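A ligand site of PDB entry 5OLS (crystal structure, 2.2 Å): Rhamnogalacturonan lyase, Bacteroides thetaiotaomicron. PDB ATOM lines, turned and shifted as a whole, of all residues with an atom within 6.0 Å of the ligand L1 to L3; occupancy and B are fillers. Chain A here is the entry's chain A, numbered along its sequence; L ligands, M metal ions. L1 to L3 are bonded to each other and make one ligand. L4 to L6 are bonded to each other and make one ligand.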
ATOM      1  N   ASN A  59      13.426  18.415 -15.735  1.00  0.00           N
ATOM      2  CA  ASN A  59      12.775  17.159 -15.341  1.00  0.00           C
ATOM      3  C   ASN A  59      13.070  16.770 -13.880  1.00  0.00           C
ATOM      4  O   ASN A  59      13.533  15.662 -13.603  1.00  0.00           O
ATOM      5  CB  ASN A  59      13.218  16.040 -16.297  1.00  0.00           C
ATOM      6  CG  ASN A  59      13.005  16.398 -17.756  1.00  0.00           C
ATOM      7  OD1 ASN A  59      13.793  17.153 -18.349  1.00  0.00           O
ATOM      8  ND2 ASN A  59      11.957  15.867 -18.333  1.00  0.00           N
ATOM      9  N   LEU A  62      16.556  15.600 -13.135  1.00  0.00           N
ATOM     10  CA  LEU A  62      17.051  14.464 -13.921  1.00  0.00           C
ATOM     11  C   LEU A  62      18.303  14.848 -14.721  1.00  0.00           C
ATOM     12  O   LEU A  62      19.158  13.991 -14.971  1.00  0.00           O
ATOM     13  CB  LEU A  62      15.975  13.913 -14.858  1.00  0.00           C
ATOM     14  CG  LEU A  62      16.290  12.662 -15.699  1.00  0.00           C
ATOM     15  CD1 LEU A  62      16.843  11.517 -14.863  1.00  0.00           C
ATOM     16  CD2 LEU A  62      15.023  12.219 -16.417  1.00  0.00           C
ATOM     17  N   TYR A  63      18.426  16.130 -15.083  1.00  0.00           N
ATOM     18  CA  TYR A  63      19.488  16.646 -15.949  1.00  0.00           C
ATOM     19  C   TYR A  63      20.392  17.702 -15.300  1.00  0.00           C
ATOM     20  O   TYR A  63      19.915  18.645 -14.688  1.00  0.00           O
ATOM     21  CB  TYR A  63      18.854  17.271 -17.187  1.00  0.00           C
ATOM     22  CG  TYR A  63      18.470  16.289 -18.275  1.00  0.00           C
ATOM     23  CD1 TYR A  63      19.376  15.940 -19.271  1.00  0.00           C
ATOM     24  CD2 TYR A  63      17.181  15.735 -18.318  1.00  0.00           C
ATOM     25  CE1 TYR A  63      19.021  15.066 -20.307  1.00  0.00           C
ATOM     26  CE2 TYR A  63      16.824  14.861 -19.339  1.00  0.00           C
ATOM     27  CZ  TYR A  63      17.738  14.527 -20.320  1.00  0.00           C
ATOM     28  OH  TYR A  63      17.378  13.653 -21.314  1.00  0.00           O
ATOM     29  N   ARG A 104      21.574  12.857 -15.723  1.00  0.00           N
ATOM     30  CA  ARG A 104      21.853  12.983 -17.165  1.00  0.00           C
ATOM     31  C   ARG A 104      22.568  14.313 -17.438  1.00  0.00           C
ATOM     32  O   ARG A 104      22.511  15.229 -16.613  1.00  0.00           O
ATOM     33  CB  ARG A 104      20.556  12.940 -17.968  1.00  0.00           C
ATOM     34  CG  ARG A 104      19.847  11.600 -17.915  1.00  0.00           C
ATOM     35  CD  ARG A 104      18.603  11.644 -18.770  1.00  0.00           C
ATOM     36  NE  ARG A 104      17.838  10.400 -18.710  1.00  0.00           N
ATOM     37  CZ  ARG A 104      16.719  10.176 -19.412  1.00  0.00           C
ATOM     38  NH1 ARG A 104      16.236  11.098 -20.238  1.00  0.00           N
ATOM     39  NH2 ARG A 104      16.086   9.010 -19.296  1.00  0.00           N
ATOM     40  N   HIS A 132      18.065   2.934 -18.262  1.00  0.00           N
ATOM     41  CA  HIS A 132      17.595   3.710 -19.398  1.00  0.00           C
ATOM     42  C   HIS A 132      17.941   5.186 -19.245  1.00  0.00           C
ATOM     43  O   HIS A 132      17.333   5.879 -18.439  1.00  0.00           O
ATOM     44  CB  HIS A 132      16.084   3.561 -19.606  1.00  0.00           C
ATOM     45  CG  HIS A 132      15.531   4.512 -20.632  1.00  0.00           C
ATOM     46  ND1 HIS A 132      15.773   4.375 -21.984  1.00  0.00           N
ATOM     47  CD2 HIS A 132      14.779   5.641 -20.501  1.00  0.00           C
ATOM     48  CE1 HIS A 132      15.187   5.358 -22.644  1.00  0.00           C
ATOM     49  NE2 HIS A 132      14.577   6.137 -21.768  1.00  0.00           N
ATOM     50  N   THR A 133      18.925   5.637 -20.012  1.00  0.00           N
ATOM     51  CA  THR A 133      19.407   7.005 -19.942  1.00  0.00           C
ATOM     52  C   THR A 133      19.968   7.520 -21.278  1.00  0.00           C
ATOM     53  O   THR A 133      20.047   6.786 -22.287  1.00  0.00           O
ATOM     54  CB  THR A 133      20.474   7.119 -18.832  1.00  0.00           C
ATOM     55  OG1 THR A 133      20.652   8.498 -18.490  1.00  0.00           O
ATOM     56  CG2 THR A 133      21.802   6.514 -19.279  1.00  0.00           C
ATOM     57  N   GLN A 134      20.318   8.796 -21.250  1.00  0.00           N
ATOM     58  CA  GLN A 134      20.929   9.500 -22.383  1.00  0.00           C
ATOM     59  C   GLN A 134      21.524  10.809 -21.872  1.00  0.00           C
ATOM     60  O   GLN A 134      21.099  11.350 -20.837  1.00  0.00           O
ATOM     61  CB  GLN A 134      19.904   9.777 -23.499  1.00  0.00           C
ATOM     62  CG  GLN A 134      18.630  10.449 -23.026  1.00  0.00           C
ATOM     63  CD  GLN A 134      17.614  10.699 -24.112  1.00  0.00           C
ATOM     64  OE1 GLN A 134      16.898   9.789 -24.534  1.00  0.00           O
ATOM     65  NE2 GLN A 134      17.525  11.955 -24.555  1.00  0.00           N
ATOM     66  N   ILE A 160      24.045  11.946 -27.303  1.00  0.00           N
ATOM     67  CA  ILE A 160      23.403  12.337 -28.547  1.00  0.00           C
ATOM     68  C   ILE A 160      23.997  13.674 -29.005  1.00  0.00           C
ATOM     69  O   ILE A 160      24.324  14.551 -28.165  1.00  0.00           O
ATOM     70  CB  ILE A 160      21.862  12.511 -28.355  1.00  0.00           C
ATOM     71  CG1 ILE A 160      21.189  11.161 -28.085  1.00  0.00           C
ATOM     72  CG2 ILE A 160      21.217  13.158 -29.589  1.00  0.00           C
ATOM     73  CD1 ILE A 160      20.053  11.267 -27.091  1.00  0.00           C
ATOM     74  N   TYR A 163      19.444  16.870 -30.234  1.00  0.00           N
ATOM     75  CA  TYR A 163      18.231  16.213 -29.754  1.00  0.00           C
ATOM     76  C   TYR A 163      17.127  17.242 -29.592  1.00  0.00           C
ATOM     77  O   TYR A 163      17.187  18.079 -28.696  1.00  0.00           O
ATOM     78  CB  TYR A 163      18.554  15.533 -28.422  1.00  0.00           C
ATOM     79  CG  TYR A 163      17.456  14.663 -27.892  1.00  0.00           C
ATOM     80  CD1 TYR A 163      17.243  13.385 -28.416  1.00  0.00           C
ATOM     81  CD2 TYR A 163      16.651  15.095 -26.835  1.00  0.00           C
ATOM     82  CE1 TYR A 163      16.248  12.569 -27.924  1.00  0.00           C
ATOM     83  CE2 TYR A 163      15.635  14.278 -26.345  1.00  0.00           C
ATOM     84  CZ  TYR A 163      15.445  13.016 -26.896  1.00  0.00           C
ATOM     85  OH  TYR A 163      14.464  12.192 -26.438  1.00  0.00           O
ATOM     86  N   LEU A 165      13.326  18.208 -28.819  1.00  0.00           N
ATOM     87  CA  LEU A 165      11.985  17.950 -28.265  1.00  0.00           C
ATOM     88  C   LEU A 165      10.939  19.023 -28.631  1.00  0.00           C
ATOM     89  O   LEU A 165       9.746  18.773 -28.494  1.00  0.00           O
ATOM     90  CB  LEU A 165      12.049  17.806 -26.734  1.00  0.00           C
ATOM     91  CG  LEU A 165      12.808  16.603 -26.179  1.00  0.00           C
ATOM     92  CD1 LEU A 165      12.863  16.670 -24.665  1.00  0.00           C
ATOM     93  CD2 LEU A 165      12.188  15.279 -26.650  1.00  0.00           C
ATOM     94  N   GLY A 191      22.024   1.956 -27.479  1.00  0.00           N
ATOM     95  CA  GLY A 191      20.763   2.044 -28.208  1.00  0.00           C
ATOM     96  C   GLY A 191      20.042   3.392 -28.183  1.00  0.00           C
ATOM     97  O   GLY A 191      18.978   3.533 -28.804  1.00  0.00           O
ATOM     98  N   ASN A 192      20.589   4.362 -27.461  1.00  0.00           N
ATOM     99  CA  ASN A 192      19.986   5.689 -27.308  1.00  0.00           C
ATOM    100  C   ASN A 192      20.811   6.821 -27.936  1.00  0.00           C
ATOM    101  O   ASN A 192      20.356   7.976 -27.957  1.00  0.00           O
ATOM    102  CB  ASN A 192      19.763   5.963 -25.820  1.00  0.00           C
ATOM    103  CG  ASN A 192      18.687   5.074 -25.209  1.00  0.00           C
ATOM    104  OD1 ASN A 192      17.887   4.469 -25.899  1.00  0.00           O
ATOM    105  ND2 ASN A 192      18.659   5.015 -23.880  1.00  0.00           N
ATOM    106  N   ASP A 194      22.012   8.608 -30.898  1.00  0.00           N
ATOM    107  CA  ASP A 194      21.907   9.050 -32.281  1.00  0.00           C
ATOM    108  C   ASP A 194      22.792  10.253 -32.583  1.00  0.00           C
ATOM    109  O   ASP A 194      23.187  11.021 -31.677  1.00  0.00           O
ATOM    110  CB  ASP A 194      20.457   9.454 -32.629  1.00  0.00           C
ATOM    111  CG  ASP A 194      19.470   8.284 -32.595  1.00  0.00           C
ATOM    112  OD1 ASP A 194      19.868   7.097 -32.680  1.00  0.00           O
ATOM    113  OD2 ASP A 194      18.246   8.549 -32.489  1.00  0.00           O
ATOM    114  N   HIS A 199      12.455  14.907 -32.467  1.00  0.00           N
ATOM    115  CA  HIS A 199      11.415  14.257 -31.647  1.00  0.00           C
ATOM    116  C   HIS A 199      10.487  15.300 -31.009  1.00  0.00           C
ATOM    117  O   HIS A 199      10.276  15.323 -29.781  1.00  0.00           O
ATOM    118  CB  HIS A 199      12.049  13.374 -30.576  1.00  0.00           C
ATOM    119  CG  HIS A 199      13.157  12.510 -31.096  1.00  0.00           C
ATOM    120  ND1 HIS A 199      12.946  11.531 -32.029  1.00  0.00           N
ATOM    121  CD2 HIS A 199      14.476  12.517 -30.831  1.00  0.00           C
ATOM    122  CE1 HIS A 199      14.094  10.948 -32.312  1.00  0.00           C
ATOM    123  NE2 HIS A 199      15.043  11.526 -31.596  1.00  0.00           N
ATOM    124  N   ASP A 229      17.207  10.250 -36.795  1.00  0.00           N
ATOM    125  CA  ASP A 229      16.036   9.576 -36.232  1.00  0.00           C
ATOM    126  C   ASP A 229      14.930  10.606 -35.971  1.00  0.00           C
ATOM    127  O   ASP A 229      15.153  11.582 -35.236  1.00  0.00           O
ATOM    128  CB  ASP A 229      16.465   8.878 -34.938  1.00  0.00           C
ATOM    129  CG  ASP A 229      15.346   8.095 -34.254  1.00  0.00           C
ATOM    130  OD1 ASP A 229      14.168   8.205 -34.661  1.00  0.00           O
ATOM    131  OD2 ASP A 229      15.681   7.367 -33.276  1.00  0.00           O
ATOM    132  N   ILE A 231      11.643   9.604 -34.835  1.00  0.00           N
ATOM    133  CA  ILE A 231      10.579   8.915 -34.139  1.00  0.00           C
ATOM    134  C   ILE A 231       9.939   9.899 -33.176  1.00  0.00           C
ATOM    135  O   ILE A 231      10.607  10.814 -32.695  1.00  0.00           O
ATOM    136  CB  ILE A 231      11.088   7.646 -33.399  1.00  0.00           C
ATOM    137  CG1 ILE A 231       9.953   6.620 -33.277  1.00  0.00           C
ATOM    138  CG2 ILE A 231      11.691   7.998 -32.031  1.00  0.00           C
ATOM    139  CD1 ILE A 231      10.317   5.360 -32.511  1.00  0.00           C
ATOM    140  N   ASN A 232       8.649   9.696 -32.916  1.00  0.00           N
ATOM    141  CA  ASN A 232       7.888  10.476 -31.950  1.00  0.00           C
ATOM    142  C   ASN A 232       8.084  11.953 -32.241  1.00  0.00           C
ATOM    143  O   ASN A 232       8.524  12.715 -31.379  1.00  0.00           O
ATOM    144  CB  ASN A 232       8.287  10.090 -30.520  1.00  0.00           C
ATOM    145  CG  ASN A 232       7.955   8.643 -30.195  1.00  0.00           C
ATOM    146  OD1 ASN A 232       6.931   8.137 -30.634  1.00  0.00           O
ATOM    147  ND2 ASN A 232       8.808   7.985 -29.450  1.00  0.00           N
HETATM  148  C1  LIG L   1      13.094   6.375 -27.413  1.00  0.00           C
HETATM  149  C2  LIG L   1      13.352   6.805 -25.964  1.00  0.00           C
HETATM  150  C3  LIG L   1      14.767   7.337 -25.865  1.00  0.00           C
HETATM  151  C4  LIG L   1      15.071   8.390 -26.929  1.00  0.00           C
HETATM  152  C5  LIG L   1      14.667   7.947 -28.330  1.00  0.00           C
HETATM  153  C6  LIG L   1      14.758   9.090 -29.335  1.00  0.00           C
HETATM  154  O1  LIG L   1      13.958   5.284 -27.738  1.00  0.00           O
HETATM  155  O2  LIG L   1      12.427   7.844 -25.611  1.00  0.00           O
HETATM  156  O3  LIG L   1      14.986   7.897 -24.571  1.00  0.00           O
HETATM  157  O4  LIG L   1      16.476   8.659 -26.906  1.00  0.00           O
HETATM  158  O5  LIG L   1      13.316   7.476 -28.310  1.00  0.00           O
HETATM  159  C1  LG2 L   2      11.617   7.620 -24.427  1.00  0.00           C
HETATM  160  C2  LG2 L   2      10.346   8.446 -24.574  1.00  0.00           C
HETATM  161  C3  LG2 L   2      10.654   9.940 -24.532  1.00  0.00           C
HETATM  162  C4  LG2 L   2      11.453  10.327 -23.298  1.00  0.00           C
HETATM  163  C5  LG2 L   2      12.653   9.370 -23.187  1.00  0.00           C
HETATM  164  C6  LG2 L   2      13.578   9.613 -22.030  1.00  0.00           C
HETATM  165  O1  LG2 L   2       9.717   8.123 -25.817  1.00  0.00           O
HETATM  166  O2  LG2 L   2       9.404  10.648 -24.554  1.00  0.00           O
HETATM  167  O3  LG2 L   2      10.538  10.224 -22.213  1.00  0.00           O
HETATM  168  O4  LG2 L   2      12.213   8.005 -23.181  1.00  0.00           O
HETATM  169  O5  LG2 L   2      13.682   8.718 -21.162  1.00  0.00           O
HETATM  170  O6  LG2 L   2      14.241  10.670 -22.000  1.00  0.00           O
HETATM  171  C1  LG3 L   3      10.225  11.361 -21.442  1.00  0.00           C
HETATM  172  C2  LG3 L   3       8.810  11.424 -20.985  1.00  0.00           C
HETATM  173  C3  LG3 L   3       8.710  10.561 -19.750  1.00  0.00           C
HETATM  174  C4  LG3 L   3       9.808  10.915 -18.752  1.00  0.00           C
HETATM  175  C5  LG3 L   3      11.194  11.244 -19.372  1.00  0.00           C
HETATM  176  C6  LG3 L   3      12.049  11.978 -18.342  1.00  0.00           C
HETATM  177  O1  LG3 L   3       8.450  12.793 -20.691  1.00  0.00           O
HETATM  178  O2  LG3 L   3       7.400  10.736 -19.204  1.00  0.00           O
HETATM  179  O3  LG3 L   3       9.966   9.774 -17.897  1.00  0.00           O
HETATM  180  O4  LG3 L   3      11.149  11.995 -20.616  1.00  0.00           O
HETATM  181  C1  LG4 L   4      15.732  -4.412 -34.814  1.00  0.00           C
HETATM  182  C2  LG4 L   4      15.952  -3.668 -33.508  1.00  0.00           C
HETATM  183  C3  LG4 L   4      14.616  -3.653 -32.757  1.00  0.00           C
HETATM  184  C4  LG4 L   4      13.541  -2.964 -33.598  1.00  0.00           C
HETATM  185  C5  LG4 L   4      13.511  -3.525 -35.048  1.00  0.00           C
HETATM  186  C6  LG4 L   4      12.610  -2.715 -35.957  1.00  0.00           C
HETATM  187  O1  LG4 L   4      16.993  -4.605 -35.450  1.00  0.00           O
HETATM  188  O2  LG4 L   4      17.007  -4.231 -32.726  1.00  0.00           O
HETATM  189  O3  LG4 L   4      14.803  -2.960 -31.504  1.00  0.00           O
HETATM  190  O4  LG4 L   4      13.908  -1.551 -33.506  1.00  0.00           O
HETATM  191  O5  LG4 L   4      14.839  -3.608 -35.614  1.00  0.00           O
HETATM  192  O6  LG4 L   4      13.136  -1.853 -36.688  1.00  0.00           O
HETATM  193  O7  LG4 L   4      11.372  -2.920 -35.975  1.00  0.00           O
HETATM  194  C1  LG5 L   5      12.849  -0.544 -33.473  1.00  0.00           C
HETATM  195  C2  LG5 L   5      13.283   0.896 -33.182  1.00  0.00           C
HETATM  196  C3  LG5 L   5      12.344   1.675 -34.108  1.00  0.00           C
HETATM  197  C4  LG5 L   5      10.897   1.446 -33.688  1.00  0.00           C
HETATM  198  C5  LG5 L   5      10.566  -0.062 -33.704  1.00  0.00           C
HETATM  199  C6  LG5 L   5       9.190  -0.378 -33.168  1.00  0.00           C
HETATM  200  O1  LG5 L   5      13.086   1.213 -31.762  1.00  0.00           O
HETATM  201  O2  LG5 L   5      12.686   3.057 -34.132  1.00  0.00           O
HETATM  202  O3  LG5 L   5      10.022   2.208 -34.543  1.00  0.00           O
HETATM  203  O4  LG5 L   5      11.535  -0.822 -32.966  1.00  0.00           O
HETATM  204  O1  LG6 L   6      14.242   5.933 -31.555  1.00  0.00           O
HETATM  205  C1  LG6 L   6      14.866   4.766 -31.508  1.00  0.00           C
HETATM  206  O2  LG6 L   6      15.978   4.666 -32.034  1.00  0.00           O
HETATM  207  C2  LG6 L   6      14.319   3.724 -30.884  1.00  0.00           C
HETATM  208  O3  LG6 L   6      15.043   2.461 -30.881  1.00  0.00           O
HETATM  209  C3  LG6 L   6      13.125   3.800 -30.246  1.00  0.00           C
HETATM  210  C4  LG6 L   6      12.607   2.650 -29.390  1.00  0.00           C
HETATM  211  O4  LG6 L   6      12.422   3.107 -28.042  1.00  0.00           O
HETATM  212  C5  LG6 L   6      13.560   1.454 -29.390  1.00  0.00           C
HETATM  213  O5  LG6 L   6      12.823   0.287 -28.986  1.00  0.00           O
HETATM  214  C6  LG6 L   6      14.188   1.313 -30.776  1.00  0.00           C
HETATM  215 CA    CA M   1      17.356   2.728 -30.420  1.00  0.00          CA
HETATM  216 CA    CA M   2      17.738   6.153 -32.616  1.00  0.00          CA
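Merely in contact with the ligand L1 to L3: His 199 (3.3 Å), Leu 62 (3.6 Å), Asn 232 (3.7 Å), Tyr 163 (3.9 Å) and Asn 59 (3.9 Å).
The nearest printed residue that does not touch the ligand L1 to L3 is Asn 192 (4.1 Å).
A ring nitrogen (NE2) of His 132 lies within hydrogen-bond range of an oxygen (O5) of LG2 L2, at 2.8 Å.
The guanidinium group (NH1) of Arg 104 lies within salt-bridge range of an oxygen (O6) of LG2 L2.
The side-chain amide oxygen (OE1) of Gln 134 sits at hydrogen-bond distance from an oxygen (O4) of LIG L1 (2.7 Å).
O1 of LIG L1 sits at hydrogen-bond distance from O4 of LG6 L6.
NE of Arg 104 sits close to OG1 of Thr 133 (3.4 Å).
OH of Tyr 63 is in hydrogen-bond range of NH1 of Arg 104 (3.0 Å).
NH2 of Arg 104 sits at hydrogen-bond distance from O of His 132 (3.5 Å).
ND1 of His 199 lies within hydrogen-bond range of O of Ile 231, at 2.5 Å.
N of Arg 104 sits at hydrogen-bond distance from O of Leu 62, 2.8 Å away.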
